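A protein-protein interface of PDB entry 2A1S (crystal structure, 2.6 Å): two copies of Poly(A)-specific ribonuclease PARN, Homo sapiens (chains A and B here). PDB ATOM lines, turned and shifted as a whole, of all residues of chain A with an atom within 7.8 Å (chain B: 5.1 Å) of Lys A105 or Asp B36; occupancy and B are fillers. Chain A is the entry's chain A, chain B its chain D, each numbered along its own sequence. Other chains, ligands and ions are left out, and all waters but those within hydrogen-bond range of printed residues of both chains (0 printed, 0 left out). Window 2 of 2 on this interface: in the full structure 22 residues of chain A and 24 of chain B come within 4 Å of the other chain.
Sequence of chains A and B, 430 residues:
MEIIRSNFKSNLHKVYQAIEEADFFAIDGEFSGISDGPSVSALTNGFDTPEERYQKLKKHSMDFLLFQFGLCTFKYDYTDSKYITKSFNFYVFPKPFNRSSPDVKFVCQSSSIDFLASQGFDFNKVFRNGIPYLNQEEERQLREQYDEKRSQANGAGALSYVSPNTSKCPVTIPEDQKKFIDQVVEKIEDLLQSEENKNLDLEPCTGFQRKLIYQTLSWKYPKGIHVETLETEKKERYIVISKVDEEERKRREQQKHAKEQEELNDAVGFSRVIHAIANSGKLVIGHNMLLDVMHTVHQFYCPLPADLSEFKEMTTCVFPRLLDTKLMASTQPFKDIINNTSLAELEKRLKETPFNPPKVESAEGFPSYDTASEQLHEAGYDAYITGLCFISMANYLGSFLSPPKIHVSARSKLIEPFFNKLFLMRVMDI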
ATOM      1  N   MET A  62      -0.499  -4.401  -1.309  1.00  0.00           N
ATOM      2  CA  MET A  62      -1.833  -4.079  -1.812  1.00  0.00           C
ATOM      3  C   MET A  62      -2.437  -5.152  -2.709  1.00  0.00           C
ATOM      4  O   MET A  62      -3.610  -5.055  -3.105  1.00  0.00           O
ATOM      5  CB  MET A  62      -1.817  -2.730  -2.513  1.00  0.00           C
ATOM      6  CG  MET A  62      -1.453  -1.575  -1.599  1.00  0.00           C
ATOM      7  SD  MET A  62      -2.263  -1.624   0.024  1.00  0.00           S
ATOM      8  CE  MET A  62      -3.679  -1.192  -0.437  1.00  0.00           C
ATOM      9  N   ASP A  63      -1.658  -6.184  -3.015  1.00  0.00           N
ATOM     10  CA  ASP A  63      -2.199  -7.346  -3.718  1.00  0.00           C
ATOM     11  C   ASP A  63      -2.875  -8.338  -2.763  1.00  0.00           C
ATOM     12  O   ASP A  63      -3.424  -9.346  -3.199  1.00  0.00           O
ATOM     13  CB  ASP A  63      -1.124  -8.031  -4.567  1.00  0.00           C
ATOM     14  CG  ASP A  63      -0.697  -7.181  -5.750  1.00  0.00           C
ATOM     15  OD1 ASP A  63      -1.529  -7.019  -6.666  1.00  0.00           O
ATOM     16  OD2 ASP A  63       0.425  -6.614  -5.849  1.00  0.00           O
ATOM     17  N   PHE A  64      -2.817  -8.050  -1.469  1.00  0.00           N
ATOM     18  CA  PHE A  64      -3.646  -8.725  -0.491  1.00  0.00           C
ATOM     19  C   PHE A  64      -5.007  -8.017  -0.390  1.00  0.00           C
ATOM     20  O   PHE A  64      -5.129  -6.830  -0.638  1.00  0.00           O
ATOM     21  CB  PHE A  64      -2.947  -8.775   0.875  1.00  0.00           C
ATOM     22  CG  PHE A  64      -1.736  -9.673   0.899  1.00  0.00           C
ATOM     23  CD1 PHE A  64      -0.462  -9.161   0.869  1.00  0.00           C
ATOM     24  CD2 PHE A  64      -1.879 -11.037   0.920  1.00  0.00           C
ATOM     25  CE1 PHE A  64       0.638  -9.996   0.886  1.00  0.00           C
ATOM     26  CE2 PHE A  64      -0.774 -11.868   0.936  1.00  0.00           C
ATOM     27  CZ  PHE A  64       0.478 -11.346   0.922  1.00  0.00           C
ATOM     28  N   LEU A  65      -6.021  -8.771  -0.006  1.00  0.00           N
ATOM     29  CA  LEU A  65      -7.365  -8.257   0.164  1.00  0.00           C
ATOM     30  C   LEU A  65      -7.624  -7.795   1.579  1.00  0.00           C
ATOM     31  O   LEU A  65      -7.256  -8.481   2.519  1.00  0.00           O
ATOM     32  CB  LEU A  65      -8.339  -9.382  -0.090  1.00  0.00           C
ATOM     33  CG  LEU A  65      -9.431  -9.110  -1.083  1.00  0.00           C
ATOM     34  CD1 LEU A  65      -8.869  -8.540  -2.381  1.00  0.00           C
ATOM     35  CD2 LEU A  65     -10.162 -10.454  -1.283  1.00  0.00           C
ATOM     36  N   PRO A  94     -14.563  -8.932  -4.094  1.00  0.00           N
ATOM     37  CA  PRO A  94     -14.805  -8.453  -5.454  1.00  0.00           C
ATOM     38  C   PRO A  94     -15.163  -9.584  -6.403  1.00  0.00           C
ATOM     39  O   PRO A  94     -14.506 -10.607  -6.422  1.00  0.00           O
ATOM     40  CB  PRO A  94     -13.461  -7.855  -5.846  1.00  0.00           C
ATOM     41  CG  PRO A  94     -12.458  -8.701  -5.116  1.00  0.00           C
ATOM     42  CD  PRO A  94     -13.130  -9.207  -3.868  1.00  0.00           C
ATOM     43  N   PRO A 102     -13.317  -6.739 -14.441  1.00  0.00           N
ATOM     44  CA  PRO A 102     -11.995  -7.264 -14.089  1.00  0.00           C
ATOM     45  C   PRO A 102     -12.099  -8.437 -13.108  1.00  0.00           C
ATOM     46  O   PRO A 102     -12.888  -8.388 -12.169  1.00  0.00           O
ATOM     47  CB  PRO A 102     -11.300  -6.065 -13.434  1.00  0.00           C
ATOM     48  CG  PRO A 102     -12.393  -5.230 -12.916  1.00  0.00           C
ATOM     49  CD  PRO A 102     -13.543  -5.408 -13.853  1.00  0.00           C
ATOM     50  N   ASP A 103     -11.324  -9.483 -13.356  1.00  0.00           N
ATOM     51  CA  ASP A 103     -11.279 -10.670 -12.510  1.00  0.00           C
ATOM     52  C   ASP A 103     -10.085 -10.538 -11.571  1.00  0.00           C
ATOM     53  O   ASP A 103      -8.950 -10.815 -11.969  1.00  0.00           O
ATOM     54  CB  ASP A 103     -11.124 -11.892 -13.412  1.00  0.00           C
ATOM     55  CG  ASP A 103     -11.365 -13.189 -12.709  1.00  0.00           C
ATOM     56  OD1 ASP A 103     -11.301 -14.203 -13.411  1.00  0.00           O
ATOM     57  OD2 ASP A 103     -11.627 -13.323 -11.492  1.00  0.00           O
ATOM     58  N   VAL A 104     -10.334 -10.105 -10.336  1.00  0.00           N
ATOM     59  CA  VAL A 104      -9.252  -9.808  -9.396  1.00  0.00           C
ATOM     60  C   VAL A 104      -8.488 -11.058  -8.977  1.00  0.00           C
ATOM     61  O   VAL A 104      -9.090 -12.074  -8.686  1.00  0.00           O
ATOM     62  CB  VAL A 104      -9.749  -9.111  -8.110  1.00  0.00           C
ATOM     63  CG1 VAL A 104      -8.584  -8.506  -7.317  1.00  0.00           C
ATOM     64  CG2 VAL A 104     -10.761  -8.032  -8.443  1.00  0.00           C
ATOM     65  N   LYS A 105      -7.160 -10.967  -8.964  1.00  0.00           N
ATOM     66  CA  LYS A 105      -6.290 -12.006  -8.430  1.00  0.00           C
ATOM     67  C   LYS A 105      -5.669 -11.401  -7.221  1.00  0.00           C
ATOM     68  O   LYS A 105      -5.062 -10.364  -7.323  1.00  0.00           O
ATOM     69  CB  LYS A 105      -5.176 -12.388  -9.413  1.00  0.00           C
ATOM     70  CG  LYS A 105      -5.668 -13.169 -10.635  1.00  0.00           C
ATOM     71  CD  LYS A 105      -5.915 -12.237 -11.832  1.00  0.00           C
ATOM     72  CE  LYS A 105      -6.735 -12.912 -12.926  1.00  0.00           C
ATOM     73  NZ  LYS A 105      -6.725 -12.072 -14.153  1.00  0.00           N
ATOM     74  N   PHE A 106      -5.849 -12.013  -6.064  1.00  0.00           N
ATOM     75  CA  PHE A 106      -5.255 -11.489  -4.844  1.00  0.00           C
ATOM     76  C   PHE A 106      -4.407 -12.583  -4.210  1.00  0.00           C
ATOM     77  O   PHE A 106      -4.460 -13.739  -4.607  1.00  0.00           O
ATOM     78  CB  PHE A 106      -6.336 -10.979  -3.877  1.00  0.00           C
ATOM     79  CG  PHE A 106      -7.338 -12.009  -3.522  1.00  0.00           C
ATOM     80  CD1 PHE A 106      -7.166 -12.806  -2.403  1.00  0.00           C
ATOM     81  CD2 PHE A 106      -8.417 -12.243  -4.345  1.00  0.00           C
ATOM     82  CE1 PHE A 106      -8.084 -13.813  -2.092  1.00  0.00           C
ATOM     83  CE2 PHE A 106      -9.341 -13.241  -4.044  1.00  0.00           C
ATOM     84  CZ  PHE A 106      -9.172 -14.022  -2.906  1.00  0.00           C
ATOM     85  N   VAL A 107      -3.638 -12.201  -3.208  1.00  0.00           N
ATOM     86  CA  VAL A 107      -2.706 -13.100  -2.553  1.00  0.00           C
ATOM     87  C   VAL A 107      -3.225 -13.398  -1.148  1.00  0.00           C
ATOM     88  O   VAL A 107      -4.020 -12.632  -0.596  1.00  0.00           O
ATOM     89  CB  VAL A 107      -1.297 -12.445  -2.495  1.00  0.00           C
ATOM     90  CG1 VAL A 107      -0.245 -13.394  -1.923  1.00  0.00           C
ATOM     91  CG2 VAL A 107      -0.877 -11.949  -3.902  1.00  0.00           C
ATOM     92  N   ILE B  34      -6.616 -20.364 -11.663  1.00  0.00           N
ATOM     93  CA  ILE B  34      -6.068 -20.940 -12.893  1.00  0.00           C
ATOM     94  C   ILE B  34      -4.846 -20.176 -13.430  1.00  0.00           C
ATOM     95  O   ILE B  34      -3.775 -20.751 -13.577  1.00  0.00           O
ATOM     96  CB  ILE B  34      -7.162 -21.008 -13.965  1.00  0.00           C
ATOM     97  CG1 ILE B  34      -8.346 -21.797 -13.415  1.00  0.00           C
ATOM     98  CG2 ILE B  34      -6.625 -21.677 -15.227  1.00  0.00           C
ATOM     99  CD1 ILE B  34      -9.544 -21.809 -14.294  1.00  0.00           C
ATOM    100  N   SER B  35      -5.005 -18.898 -13.758  1.00  0.00           N
ATOM    101  CA  SER B  35      -3.872 -18.080 -14.218  1.00  0.00           C
ATOM    102  C   SER B  35      -3.929 -16.660 -13.697  1.00  0.00           C
ATOM    103  O   SER B  35      -4.996 -16.079 -13.548  1.00  0.00           O
ATOM    104  CB  SER B  35      -3.786 -18.075 -15.731  1.00  0.00           C
ATOM    105  OG  SER B  35      -4.050 -19.369 -16.221  1.00  0.00           O
ATOM    106  N   ASP B  36      -2.755 -16.103 -13.431  1.00  0.00           N
ATOM    107  CA  ASP B  36      -2.649 -14.796 -12.777  1.00  0.00           C
ATOM    108  C   ASP B  36      -2.651 -13.611 -13.752  1.00  0.00           C
ATOM    109  O   ASP B  36      -2.421 -12.474 -13.333  1.00  0.00           O
ATOM    110  CB  ASP B  36      -1.387 -14.754 -11.910  1.00  0.00           C
ATOM    111  CG  ASP B  36      -0.138 -15.098 -12.694  1.00  0.00           C
ATOM    112  OD1 ASP B  36       0.853 -15.542 -12.068  1.00  0.00           O
ATOM    113  OD2 ASP B  36      -0.072 -14.974 -13.943  1.00  0.00           O
ATOM    114  N   GLY B  37      -2.897 -13.872 -15.039  1.00  0.00           N
ATOM    115  CA  GLY B  37      -2.943 -12.817 -16.044  1.00  0.00           C
ATOM    116  C   GLY B  37      -3.343 -13.261 -17.449  1.00  0.00           C
ATOM    117  O   GLY B  37      -4.456 -12.968 -17.890  1.00  0.00           O
ATOM    118  N   PRO B  38      -2.437 -13.944 -18.157  1.00  0.00           N
ATOM    119  CA  PRO B  38      -2.696 -14.368 -19.550  1.00  0.00           C
ATOM    120  C   PRO B  38      -3.861 -15.359 -19.696  1.00  0.00           C
ATOM    121  O   PRO B  38      -4.365 -15.518 -20.815  1.00  0.00           O
ATOM    122  CB  PRO B  38      -1.360 -15.016 -19.996  1.00  0.00           C
ATOM    123  CG  PRO B  38      -0.591 -15.323 -18.713  1.00  0.00           C
ATOM    124  CD  PRO B  38      -1.089 -14.337 -17.689  1.00  0.00           C
ATOM    125  N   LYS B  59       5.069 -20.904 -14.228  1.00  0.00           N
ATOM    126  CA  LYS B  59       5.149 -19.529 -13.759  1.00  0.00           C
ATOM    127  C   LYS B  59       3.799 -18.924 -13.329  1.00  0.00           C
ATOM    128  O   LYS B  59       3.752 -18.168 -12.368  1.00  0.00           O
ATOM    129  CB  LYS B  59       5.761 -18.664 -14.868  1.00  0.00           C
ATOM    130  CG  LYS B  59       6.169 -17.249 -14.452  1.00  0.00           C
ATOM    131  CD  LYS B  59       6.904 -16.529 -15.581  1.00  0.00           C
ATOM    132  CE  LYS B  59       8.213 -17.236 -15.998  1.00  0.00           C
ATOM    133  NZ  LYS B  59       9.077 -17.592 -14.825  1.00  0.00           N
ATOM    134  N   HIS B  60       2.718 -19.229 -14.039  1.00  0.00           N
ATOM    135  CA  HIS B  60       1.464 -18.480 -13.875  1.00  0.00           C
ATOM    136  C   HIS B  60       0.285 -19.312 -13.377  1.00  0.00           C
ATOM    137  O   HIS B  60      -0.820 -18.812 -13.278  1.00  0.00           O
ATOM    138  CB  HIS B  60       1.084 -17.797 -15.197  1.00  0.00           C
ATOM    139  CG  HIS B  60       2.096 -16.805 -15.667  1.00  0.00           C
ATOM    140  ND1 HIS B  60       2.703 -16.891 -16.899  1.00  0.00           N
ATOM    141  CD2 HIS B  60       2.625 -15.715 -15.061  1.00  0.00           C
ATOM    142  CE1 HIS B  60       3.555 -15.893 -17.036  1.00  0.00           C
ATOM    143  NE2 HIS B  60       3.523 -15.162 -15.938  1.00  0.00           N
ATOM    144  N   PHE B  64      -1.078 -20.776  -7.494  1.00  0.00           N
ATOM    145  CA  PHE B  64      -2.399 -21.160  -7.011  1.00  0.00           C
ATOM    146  C   PHE B  64      -2.340 -22.498  -6.253  1.00  0.00           C
ATOM    147  O   PHE B  64      -1.351 -23.211  -6.289  1.00  0.00           O
ATOM    148  CB  PHE B  64      -3.398 -21.278  -8.170  1.00  0.00           C
ATOM    149  CG  PHE B  64      -3.644 -19.992  -8.915  1.00  0.00           C
ATOM    150  CD1 PHE B  64      -3.107 -19.790 -10.173  1.00  0.00           C
ATOM    151  CD2 PHE B  64      -4.427 -19.004  -8.378  1.00  0.00           C
ATOM    152  CE1 PHE B  64      -3.345 -18.611 -10.870  1.00  0.00           C
ATOM    153  CE2 PHE B  64      -4.675 -17.817  -9.091  1.00  0.00           C
ATOM    154  CZ  PHE B  64      -4.134 -17.627 -10.329  1.00  0.00           C
ATOM    155  N   VAL B 107      -2.033 -17.548  -4.471  1.00  0.00           N
ATOM    156  CA  VAL B 107      -2.887 -16.594  -5.187  1.00  0.00           C
ATOM    157  C   VAL B 107      -4.292 -17.149  -5.376  1.00  0.00           C
ATOM    158  O   VAL B 107      -4.477 -18.361  -5.463  1.00  0.00           O
ATOM    159  CB  VAL B 107      -2.305 -16.283  -6.576  1.00  0.00           C
ATOM    160  CG1 VAL B 107      -2.894 -15.049  -7.141  1.00  0.00           C
ATOM    161  CG2 VAL B 107      -0.809 -16.098  -6.477  1.00  0.00           C
ATOM    162  N   CYS B 108      -5.274 -16.257  -5.467  1.00  0.00           N
ATOM    163  CA  CYS B 108      -6.657 -16.639  -5.729  1.00  0.00           C
ATOM    164  C   CYS B 108      -7.276 -15.844  -6.873  1.00  0.00           C
ATOM    165  O   CYS B 108      -7.048 -14.639  -7.022  1.00  0.00           O
ATOM    166  CB  CYS B 108      -7.492 -16.403  -4.488  1.00  0.00           C
ATOM    167  SG  CYS B 108      -7.066 -17.488  -3.130  1.00  0.00           S
ATOM    168  N   GLN B 109      -8.085 -16.536  -7.668  1.00  0.00           N
ATOM    169  CA  GLN B 109      -8.742 -15.936  -8.800  1.00  0.00           C
ATOM    170  C   GLN B 109     -10.179 -15.758  -8.389  1.00  0.00           C
ATOM    171  O   GLN B 109     -10.866 -16.741  -8.158  1.00  0.00           O
ATOM    172  CB  GLN B 109      -8.623 -16.825 -10.040  1.00  0.00           C
ATOM    173  CG  GLN B 109      -8.177 -16.042 -11.264  1.00  0.00           C
ATOM    174  CD  GLN B 109      -8.278 -16.832 -12.552  1.00  0.00           C
ATOM    175  OE1 GLN B 109      -7.644 -17.877 -12.714  1.00  0.00           O
ATOM    176  NE2 GLN B 109      -9.054 -16.319 -13.482  1.00  0.00           N
ATOM    177  N   SER B 110     -10.627 -14.510  -8.274  1.00  0.00           N
ATOM    178  CA  SER B 110     -11.997 -14.233  -7.869  1.00  0.00           C
ATOM    179  C   SER B 110     -13.074 -15.064  -8.610  1.00  0.00           C
ATOM    180  O   SER B 110     -14.026 -15.500  -7.993  1.00  0.00           O
ATOM    181  CB  SER B 110     -12.282 -12.750  -8.005  1.00  0.00           C
ATOM    182  OG  SER B 110     -11.619 -12.050  -6.979  1.00  0.00           O
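Among the printed residues, pairs that only touch across the chains: Asp A103 with Ser B110 (3.6 Å), Val A104 with Cys B108 (3.7 Å), Val A104 with Gln B109 (3.9 Å), Lys A105 with Ser B35 (3.7 Å), Lys A105 with Asp B36 (3.8 Å), Lys A105 with Cys B108 (3.1 Å), Lys A105 with Gln B109 (3.8 Å), Phe A106 with Val B107 (3.3 Å) and Phe A106 with Ser B110 (3.9 Å).
2 positions are printed for both chains.
The side-chain amino group (NZ) of Lys A105 sits close to the backbone carbonyl oxygen (O) of Asp A103 (3.4 Å).
The backbone NH (N) of Ile B34 sits at hydrogen-bond distance from the side-chain amide oxygen (OE1) of Gln B109.
The backbone NH (N) of Ser B35 lies within hydrogen-bond range of the side-chain amide oxygen (OE1) of Gln B109.
The backbone carbonyl oxygen (O) of His B60 lies within hydrogen-bond range of the backbone NH (N) of Asp B36.
Printed residues of chain B within 4 Å of Pro A94: Ser B110 (3.3 Å).
Lys A105 touches just these residues of chain B: Ser B35, Asp B36, Cys B108 and Gln B109.
Asp B36 touches one residue of chain A.
Of the printed residues of chain A, Val B107 touches Phe A106 (3.3 Å).
Printed residues of chain A within 4 Å of Cys B108: Val A104, Lys A105 and Phe A106.
Printed residues of chain A that touch a printed residue of chain B: Pro A94, Asp A103, Val A104, Lys A105 and Phe A106.
Hydrophobic or aromatic side chains of chain A within 4 Å of the printed part of chain B: Pro A94, Val A104 and Phe A106.
Of the 12 printed residues of chain B, 6 touch a printed residue of chain A.
Among the printed residues, 13 pairs touch across the chains.
Among the printed residues, no Asp or Glu carboxylate lies within 4 Å of a Lys or Arg side-chain nitrogen of the other chain.
The side-chain hydroxyl of Ser B110 sits at hydrogen-bond distance from the backbone carbonyl oxygen of Pro A94 (3.3 Å).
The side-chain amide nitrogen (NE2) of Gln B109 lies within hydrogen-bond range of the side-chain carboxylate (OD1) of Asp A103 (3.1 Å).
O of Val A104 lies within hydrogen-bond range of N of Ser B110 (2.9 Å).
O of Phe A106 sits at hydrogen-bond distance from N of Cys B108 (2.8 Å).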
